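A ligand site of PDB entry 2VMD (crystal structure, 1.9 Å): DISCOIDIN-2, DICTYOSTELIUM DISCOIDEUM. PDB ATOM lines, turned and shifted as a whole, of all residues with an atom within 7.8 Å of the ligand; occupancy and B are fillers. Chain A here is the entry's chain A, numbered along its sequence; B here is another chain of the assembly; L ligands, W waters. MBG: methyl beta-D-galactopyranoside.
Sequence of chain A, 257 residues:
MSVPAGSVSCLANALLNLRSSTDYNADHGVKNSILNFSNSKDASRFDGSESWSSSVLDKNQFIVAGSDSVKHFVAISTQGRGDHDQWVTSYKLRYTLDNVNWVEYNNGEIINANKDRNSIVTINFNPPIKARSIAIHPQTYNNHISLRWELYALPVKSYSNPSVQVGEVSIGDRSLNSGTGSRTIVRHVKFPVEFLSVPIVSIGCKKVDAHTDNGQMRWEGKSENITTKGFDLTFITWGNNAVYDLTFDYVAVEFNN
Water W2 bridges O6 of the ligand (2.8 Å) and ND2 of Asn 177 of chain B (3.2 Å).
Water W1 bridges an oxygen (O6) of the ligand (3.0 Å) and the side-chain amide oxygen of Gln 216 (3.1 Å).
The guanidinium group of Arg 218 lies within salt-bridge range of the side-chain carboxylate of Asp 213 (2.8 Å).
The side-chain carboxylate of Asp 209 of chain B sits at hydrogen-bond distance from the side-chain amide nitrogen of Gln 216.
O of Asp 209 of chain B is in hydrogen-bond range of N of Tyr 244 of chain B, 2.7 Å away.
The backbone carbonyl oxygen (O) of Asp 209 of chain B lies within hydrogen-bond range of the backbone NH (N) of Asp 245 of chain B (2.9 Å).
The side-chain amide oxygen of Asn 241 lies close to the backbone carbonyl oxygen of Trp 238 (3.3 Å).
The backbone NH (N) of Ala 210 of chain B lies close to the side-chain amide nitrogen (NE2) of Gln 216 (3.5 Å).
The side-chain amide oxygen of Gln 216 is in hydrogen-bond range of a ring nitrogen (ND1) of His 211 of chain B (2.7 Å).
The side-chain amide nitrogen of Asn 241 is in hydrogen-bond range of the backbone carbonyl oxygen of Gln 216, at 2.8 Å.
Gln 216 touches the ligand.
Tyr 244 of chain B touches the ligand (CD1 to C4, 3.6 Å).
Of the 21 residues printed, 5 come within 4 Å of the ligand.
An oxygen (O4) of the ligand is in hydrogen-bond range of the guanidinium group (NE) of Arg 218, at 2.6 Å.
OD1 of Asp 209 of chain B sits at hydrogen-bond distance from O4 of the ligand (2.7 Å).
NE1 of Trp 238 sits at hydrogen-bond distance from O3 of the ligand.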
ATOM      1  N   GLY A 181      -4.928 -13.028 -36.007  1.00  0.00           N
ATOM      2  CA  GLY A 181      -3.662 -12.506 -35.468  1.00  0.00           C
ATOM      3  C   GLY A 181      -3.870 -12.060 -34.017  1.00  0.00           C
ATOM      4  O   GLY A 181      -4.975 -12.265 -33.465  1.00  0.00           O
ATOM      5  N   SER A 182      -2.828 -11.478 -33.423  1.00  0.00           N
ATOM      6  CA  SER A 182      -2.871 -10.978 -32.034  1.00  0.00           C
ATOM      7  C   SER A 182      -3.982  -9.969 -31.858  1.00  0.00           C
ATOM      8  O   SER A 182      -4.006  -8.916 -32.527  1.00  0.00           O
ATOM      9  CB  SER A 182      -1.578 -10.301 -31.632  1.00  0.00           C
ATOM     10  OG  SER A 182      -0.494 -11.211 -31.646  1.00  0.00           O
ATOM     11  N   ASP A 213      -9.080 -22.935 -33.105  1.00  0.00           N
ATOM     12  CA  ASP A 213      -8.663 -22.552 -34.436  1.00  0.00           C
ATOM     13  C   ASP A 213      -7.904 -23.754 -34.982  1.00  0.00           C
ATOM     14  O   ASP A 213      -6.741 -24.003 -34.595  1.00  0.00           O
ATOM     15  CB  ASP A 213      -7.758 -21.319 -34.360  1.00  0.00           C
ATOM     16  CG  ASP A 213      -6.977 -21.065 -35.666  1.00  0.00           C
ATOM     17  OD1 ASP A 213      -7.469 -21.516 -36.741  1.00  0.00           O
ATOM     18  OD2 ASP A 213      -5.889 -20.406 -35.605  1.00  0.00           O
ATOM     19  N   ASN A 214      -8.589 -24.524 -35.828  1.00  0.00           N
ATOM     20  CA  ASN A 214      -8.037 -25.806 -36.301  1.00  0.00           C
ATOM     21  C   ASN A 214      -7.576 -26.674 -35.118  1.00  0.00           C
ATOM     22  O   ASN A 214      -6.446 -27.168 -35.115  1.00  0.00           O
ATOM     23  CB  ASN A 214      -6.845 -25.540 -37.275  1.00  0.00           C
ATOM     24  CG  ASN A 214      -7.307 -25.073 -38.662  1.00  0.00           C
ATOM     25  OD1 ASN A 214      -6.597 -24.331 -39.348  1.00  0.00           O
ATOM     26  ND2 ASN A 214      -8.506 -25.474 -39.047  1.00  0.00           N
ATOM     27  N   GLN A 216      -6.559 -25.716 -32.107  1.00  0.00           N
ATOM     28  CA  GLN A 216      -5.713 -25.008 -31.120  1.00  0.00           C
ATOM     29  C   GLN A 216      -6.566 -24.041 -30.304  1.00  0.00           C
ATOM     30  O   GLN A 216      -7.243 -23.192 -30.886  1.00  0.00           O
ATOM     31  CB  GLN A 216      -4.591 -24.186 -31.791  1.00  0.00           C
ATOM     32  CG  GLN A 216      -3.458 -23.811 -30.812  1.00  0.00           C
ATOM     33  CD  GLN A 216      -2.614 -25.038 -30.506  1.00  0.00           C
ATOM     34  OE1 GLN A 216      -2.770 -26.064 -31.179  1.00  0.00           O
ATOM     35  NE2 GLN A 216      -1.705 -24.940 -29.537  1.00  0.00           N
ATOM     36  N   MET A 217      -6.501 -24.131 -28.975  1.00  0.00           N
ATOM     37  CA  MET A 217      -7.097 -23.113 -28.082  1.00  0.00           C
ATOM     38  C   MET A 217      -6.006 -22.118 -27.675  1.00  0.00           C
ATOM     39  O   MET A 217      -4.878 -22.518 -27.342  1.00  0.00           O
ATOM     40  CB  MET A 217      -7.705 -23.758 -26.832  1.00  0.00           C
ATOM     41  CG  MET A 217      -8.207 -22.732 -25.829  1.00  0.00           C
ATOM     42  SD  MET A 217      -9.601 -21.868 -26.539  1.00  0.00           S
ATOM     43  CE  MET A 217     -10.843 -23.126 -26.255  1.00  0.00           C
ATOM     44  N   ARG A 218      -6.316 -20.830 -27.780  1.00  0.00           N
ATOM     45  CA  ARG A 218      -5.396 -19.749 -27.431  1.00  0.00           C
ATOM     46  C   ARG A 218      -6.138 -18.659 -26.642  1.00  0.00           C
ATOM     47  O   ARG A 218      -7.001 -17.966 -27.197  1.00  0.00           O
ATOM     48  CB  ARG A 218      -4.777 -19.152 -28.683  1.00  0.00           C
ATOM     49  CG  ARG A 218      -4.040 -20.150 -29.560  1.00  0.00           C
ATOM     50  CD  ARG A 218      -3.485 -19.423 -30.781  1.00  0.00           C
ATOM     51  NE  ARG A 218      -2.760 -20.310 -31.686  1.00  0.00           N
ATOM     52  CZ  ARG A 218      -3.250 -20.800 -32.811  1.00  0.00           C
ATOM     53  NH1 ARG A 218      -4.484 -20.489 -33.178  1.00  0.00           N
ATOM     54  NH2 ARG A 218      -2.494 -21.569 -33.599  1.00  0.00           N
ATOM     55  N   TRP A 238      -4.877 -15.008 -30.057  1.00  0.00           N
ATOM     56  CA  TRP A 238      -4.029 -14.844 -31.244  1.00  0.00           C
ATOM     57  C   TRP A 238      -4.329 -15.990 -32.211  1.00  0.00           C
ATOM     58  O   TRP A 238      -5.321 -16.706 -32.017  1.00  0.00           O
ATOM     59  CB  TRP A 238      -2.542 -14.646 -30.872  1.00  0.00           C
ATOM     60  CG  TRP A 238      -1.927 -15.821 -30.165  1.00  0.00           C
ATOM     61  CD1 TRP A 238      -1.036 -16.722 -30.694  1.00  0.00           C
ATOM     62  CD2 TRP A 238      -2.128 -16.220 -28.797  1.00  0.00           C
ATOM     63  NE1 TRP A 238      -0.668 -17.655 -29.742  1.00  0.00           N
ATOM     64  CE2 TRP A 238      -1.313 -17.362 -28.559  1.00  0.00           C
ATOM     65  CE3 TRP A 238      -2.883 -15.703 -27.731  1.00  0.00           C
ATOM     66  CZ2 TRP A 238      -1.280 -18.029 -27.308  1.00  0.00           C
ATOM     67  CZ3 TRP A 238      -2.857 -16.350 -26.487  1.00  0.00           C
ATOM     68  CH2 TRP A 238      -2.059 -17.519 -26.289  1.00  0.00           C
ATOM     69  N   GLY A 239      -3.518 -16.151 -33.257  1.00  0.00           N
ATOM     70  CA  GLY A 239      -3.949 -16.941 -34.422  1.00  0.00           C
ATOM     71  C   GLY A 239      -5.349 -16.513 -34.865  1.00  0.00           C
ATOM     72  O   GLY A 239      -5.636 -15.309 -34.935  1.00  0.00           O
ATOM     73  N   ASN A 240      -6.212 -17.475 -35.148  1.00  0.00           N
ATOM     74  CA  ASN A 240      -7.562 -17.170 -35.588  1.00  0.00           C
ATOM     75  C   ASN A 240      -8.655 -17.593 -34.606  1.00  0.00           C
ATOM     76  O   ASN A 240      -9.788 -17.828 -35.007  1.00  0.00           O
ATOM     77  CB  ASN A 240      -7.809 -17.781 -36.982  1.00  0.00           C
ATOM     78  CG  ASN A 240      -6.916 -17.164 -38.057  1.00  0.00           C
ATOM     79  OD1 ASN A 240      -6.640 -15.957 -38.053  1.00  0.00           O
ATOM     80  ND2 ASN A 240      -6.474 -18.001 -38.990  1.00  0.00           N
ATOM     81  N   ASN A 241      -8.337 -17.678 -33.313  1.00  0.00           N
ATOM     82  CA  ASN A 241      -9.365 -18.065 -32.341  1.00  0.00           C
ATOM     83  C   ASN A 241     -10.369 -16.973 -32.161  1.00  0.00           C
ATOM     84  O   ASN A 241     -10.028 -15.798 -32.258  1.00  0.00           O
ATOM     85  CB  ASN A 241      -8.757 -18.392 -30.997  1.00  0.00           C
ATOM     86  CG  ASN A 241      -7.907 -19.623 -31.031  1.00  0.00           C
ATOM     87  OD1 ASN A 241      -6.769 -19.575 -31.470  1.00  0.00           O
ATOM     88  ND2 ASN A 241      -8.441 -20.745 -30.497  1.00  0.00           N
ATOM     89  N   ARG B 174       8.481 -26.035 -25.490  1.00  0.00           N
ATOM     90  CA  ARG B 174       7.586 -27.008 -26.157  1.00  0.00           C
ATOM     91  C   ARG B 174       7.609 -28.401 -25.563  1.00  0.00           C
ATOM     92  O   ARG B 174       7.305 -29.358 -26.280  1.00  0.00           O
ATOM     93  CB  ARG B 174       7.815 -27.083 -27.667  1.00  0.00           C
ATOM     94  CG  ARG B 174       7.938 -25.743 -28.382  1.00  0.00           C
ATOM     95  CD  ARG B 174       6.612 -24.979 -28.481  1.00  0.00           C
ATOM     96  NE  ARG B 174       6.185 -24.326 -27.226  1.00  0.00           N
ATOM     97  CZ  ARG B 174       6.613 -23.138 -26.806  1.00  0.00           C
ATOM     98  NH1 ARG B 174       7.511 -22.453 -27.507  1.00  0.00           N
ATOM     99  NH2 ARG B 174       6.147 -22.639 -25.661  1.00  0.00           N
ATOM    100  N   ASN B 177       4.436 -30.252 -25.915  1.00  0.00           N
ATOM    101  CA  ASN B 177       3.816 -30.001 -27.220  1.00  0.00           C
ATOM    102  C   ASN B 177       3.749 -31.199 -28.193  1.00  0.00           C
ATOM    103  O   ASN B 177       3.467 -31.007 -29.375  1.00  0.00           O
ATOM    104  CB  ASN B 177       4.475 -28.818 -27.913  1.00  0.00           C
ATOM    105  CG  ASN B 177       3.577 -28.193 -28.959  1.00  0.00           C
ATOM    106  OD1 ASN B 177       2.385 -27.971 -28.739  1.00  0.00           O
ATOM    107  ND2 ASN B 177       4.158 -27.890 -30.119  1.00  0.00           N
ATOM    108  N   LYS B 207      -3.252 -18.519 -18.829  1.00  0.00           N
ATOM    109  CA  LYS B 207      -2.967 -18.723 -20.267  1.00  0.00           C
ATOM    110  C   LYS B 207      -3.047 -20.185 -20.658  1.00  0.00           C
ATOM    111  O   LYS B 207      -2.395 -21.035 -20.025  1.00  0.00           O
ATOM    112  CB  LYS B 207      -1.568 -18.238 -20.624  1.00  0.00           C
ATOM    113  CG  LYS B 207      -1.181 -18.553 -22.055  1.00  0.00           C
ATOM    114  CD  LYS B 207       0.332 -18.383 -22.275  1.00  0.00           C
ATOM    115  CE  LYS B 207       0.631 -18.353 -23.715  1.00  0.00           C
ATOM    116  NZ  LYS B 207       2.089 -18.024 -23.942  1.00  0.00           N
ATOM    117  N   VAL B 208      -3.805 -20.442 -21.722  1.00  0.00           N
ATOM    118  CA  VAL B 208      -3.853 -21.746 -22.376  1.00  0.00           C
ATOM    119  C   VAL B 208      -3.486 -21.582 -23.850  1.00  0.00           C
ATOM    120  O   VAL B 208      -4.094 -20.768 -24.578  1.00  0.00           O
ATOM    121  CB  VAL B 208      -5.249 -22.413 -22.238  1.00  0.00           C
ATOM    122  CG1 VAL B 208      -5.391 -23.650 -23.175  1.00  0.00           C
ATOM    123  CG2 VAL B 208      -5.488 -22.806 -20.808  1.00  0.00           C
ATOM    124  N   ASP B 209      -2.462 -22.332 -24.266  1.00  0.00           N
ATOM    125  CA  ASP B 209      -2.052 -22.483 -25.667  1.00  0.00           C
ATOM    126  C   ASP B 209      -1.878 -23.979 -25.895  1.00  0.00           C
ATOM    127  O   ASP B 209      -0.788 -24.548 -25.666  1.00  0.00           O
ATOM    128  CB  ASP B 209      -0.757 -21.730 -25.914  1.00  0.00           C
ATOM    129  CG  ASP B 209      -0.398 -21.614 -27.375  1.00  0.00           C
ATOM    130  OD1 ASP B 209      -1.091 -22.233 -28.234  1.00  0.00           O
ATOM    131  OD2 ASP B 209       0.616 -20.913 -27.668  1.00  0.00           O
ATOM    132  N   ALA B 210      -2.957 -24.632 -26.323  1.00  0.00           N
ATOM    133  CA  ALA B 210      -2.990 -26.092 -26.363  1.00  0.00           C
ATOM    134  C   ALA B 210      -3.867 -26.606 -27.502  1.00  0.00           C
ATOM    135  O   ALA B 210      -4.846 -25.964 -27.894  1.00  0.00           O
ATOM    136  CB  ALA B 210      -3.488 -26.644 -25.024  1.00  0.00           C
ATOM    137  N   HIS B 211      -3.534 -27.795 -27.982  1.00  0.00           N
ATOM    138  CA  HIS B 211      -4.321 -28.440 -29.022  1.00  0.00           C
ATOM    139  C   HIS B 211      -5.210 -29.537 -28.431  1.00  0.00           C
ATOM    140  O   HIS B 211      -4.769 -30.315 -27.570  1.00  0.00           O
ATOM    141  CB  HIS B 211      -3.382 -29.054 -30.072  1.00  0.00           C
ATOM    142  CG  HIS B 211      -3.996 -29.218 -31.428  1.00  0.00           C
ATOM    143  ND1 HIS B 211      -4.035 -28.187 -32.354  1.00  0.00           N
ATOM    144  CD2 HIS B 211      -4.626 -30.260 -32.008  1.00  0.00           C
ATOM    145  CE1 HIS B 211      -4.638 -28.612 -33.452  1.00  0.00           C
ATOM    146  NE2 HIS B 211      -5.017 -29.863 -33.264  1.00  0.00           N
ATOM    147  N   ALA B 242      -1.432 -31.885 -27.279  1.00  0.00           N
ATOM    148  CA  ALA B 242      -0.196 -31.144 -27.450  1.00  0.00           C
ATOM    149  C   ALA B 242      -0.402 -29.793 -26.783  1.00  0.00           C
ATOM    150  O   ALA B 242      -1.222 -28.998 -27.227  1.00  0.00           O
ATOM    151  CB  ALA B 242       0.105 -30.990 -28.927  1.00  0.00           C
ATOM    152  N   TYR B 244       1.201 -26.341 -25.959  1.00  0.00           N
ATOM    153  CA  TYR B 244       2.232 -25.406 -26.436  1.00  0.00           C
ATOM    154  C   TYR B 244       2.763 -24.534 -25.300  1.00  0.00           C
ATOM    155  O   TYR B 244       3.995 -24.388 -25.139  1.00  0.00           O
ATOM    156  CB  TYR B 244       1.695 -24.565 -27.589  1.00  0.00           C
ATOM    157  CG  TYR B 244       2.709 -23.773 -28.402  1.00  0.00           C
ATOM    158  CD1 TYR B 244       3.134 -24.251 -29.650  1.00  0.00           C
ATOM    159  CD2 TYR B 244       3.204 -22.551 -27.945  1.00  0.00           C
ATOM    160  CE1 TYR B 244       4.067 -23.531 -30.410  1.00  0.00           C
ATOM    161  CE2 TYR B 244       4.108 -21.816 -28.706  1.00  0.00           C
ATOM    162  CZ  TYR B 244       4.538 -22.311 -29.924  1.00  0.00           C
ATOM    163  OH  TYR B 244       5.440 -21.560 -30.668  1.00  0.00           O
ATOM    164  N   ASP B 245       1.854 -24.003 -24.477  1.00  0.00           N
ATOM    165  CA  ASP B 245       2.241 -23.302 -23.248  1.00  0.00           C
ATOM    166  C   ASP B 245       1.065 -23.236 -22.300  1.00  0.00           C
ATOM    167  O   ASP B 245      -0.086 -23.241 -22.762  1.00  0.00           O
ATOM    168  CB  ASP B 245       2.699 -21.872 -23.573  1.00  0.00           C
ATOM    169  CG  ASP B 245       3.640 -21.251 -22.510  1.00  0.00           C
ATOM    170  OD1 ASP B 245       4.165 -21.962 -21.609  1.00  0.00           O
ATOM    171  OD2 ASP B 245       3.890 -20.025 -22.611  1.00  0.00           O
HETATM  172  C1  MBG L   1       1.398 -20.663 -33.533  1.00  0.00           C
HETATM  173  C2  MBG L   1       1.123 -19.747 -32.325  1.00  0.00           C
HETATM  174  C3  MBG L   1       1.503 -20.487 -31.049  1.00  0.00           C
HETATM  175  C4  MBG L   1       0.766 -21.827 -30.965  1.00  0.00           C
HETATM  176  C5  MBG L   1       1.001 -22.606 -32.275  1.00  0.00           C
HETATM  177  C6  MBG L   1       0.244 -23.926 -32.263  1.00  0.00           C
HETATM  178  C7  MBG L   1       0.257 -18.910 -34.726  1.00  0.00           C
HETATM  179  O1  MBG L   1       1.183 -20.032 -34.816  1.00  0.00           O
HETATM  180  O2  MBG L   1       1.863 -18.522 -32.355  1.00  0.00           O
HETATM  181  O3  MBG L   1       1.253 -19.637 -29.917  1.00  0.00           O
HETATM  182  O4  MBG L   1      -0.648 -21.595 -30.779  1.00  0.00           O
HETATM  183  O5  MBG L   1       0.570 -21.854 -33.409  1.00  0.00           O
HETATM  184  O6  MBG L   1       0.722 -24.748 -33.347  1.00  0.00           O
HETATM  185  O   HOH W   1      -1.867 -25.993 -34.168  1.00  0.00           O
HETATM  186  O   HOH W   2       2.354 -26.813 -32.524  1.00  0.00           O
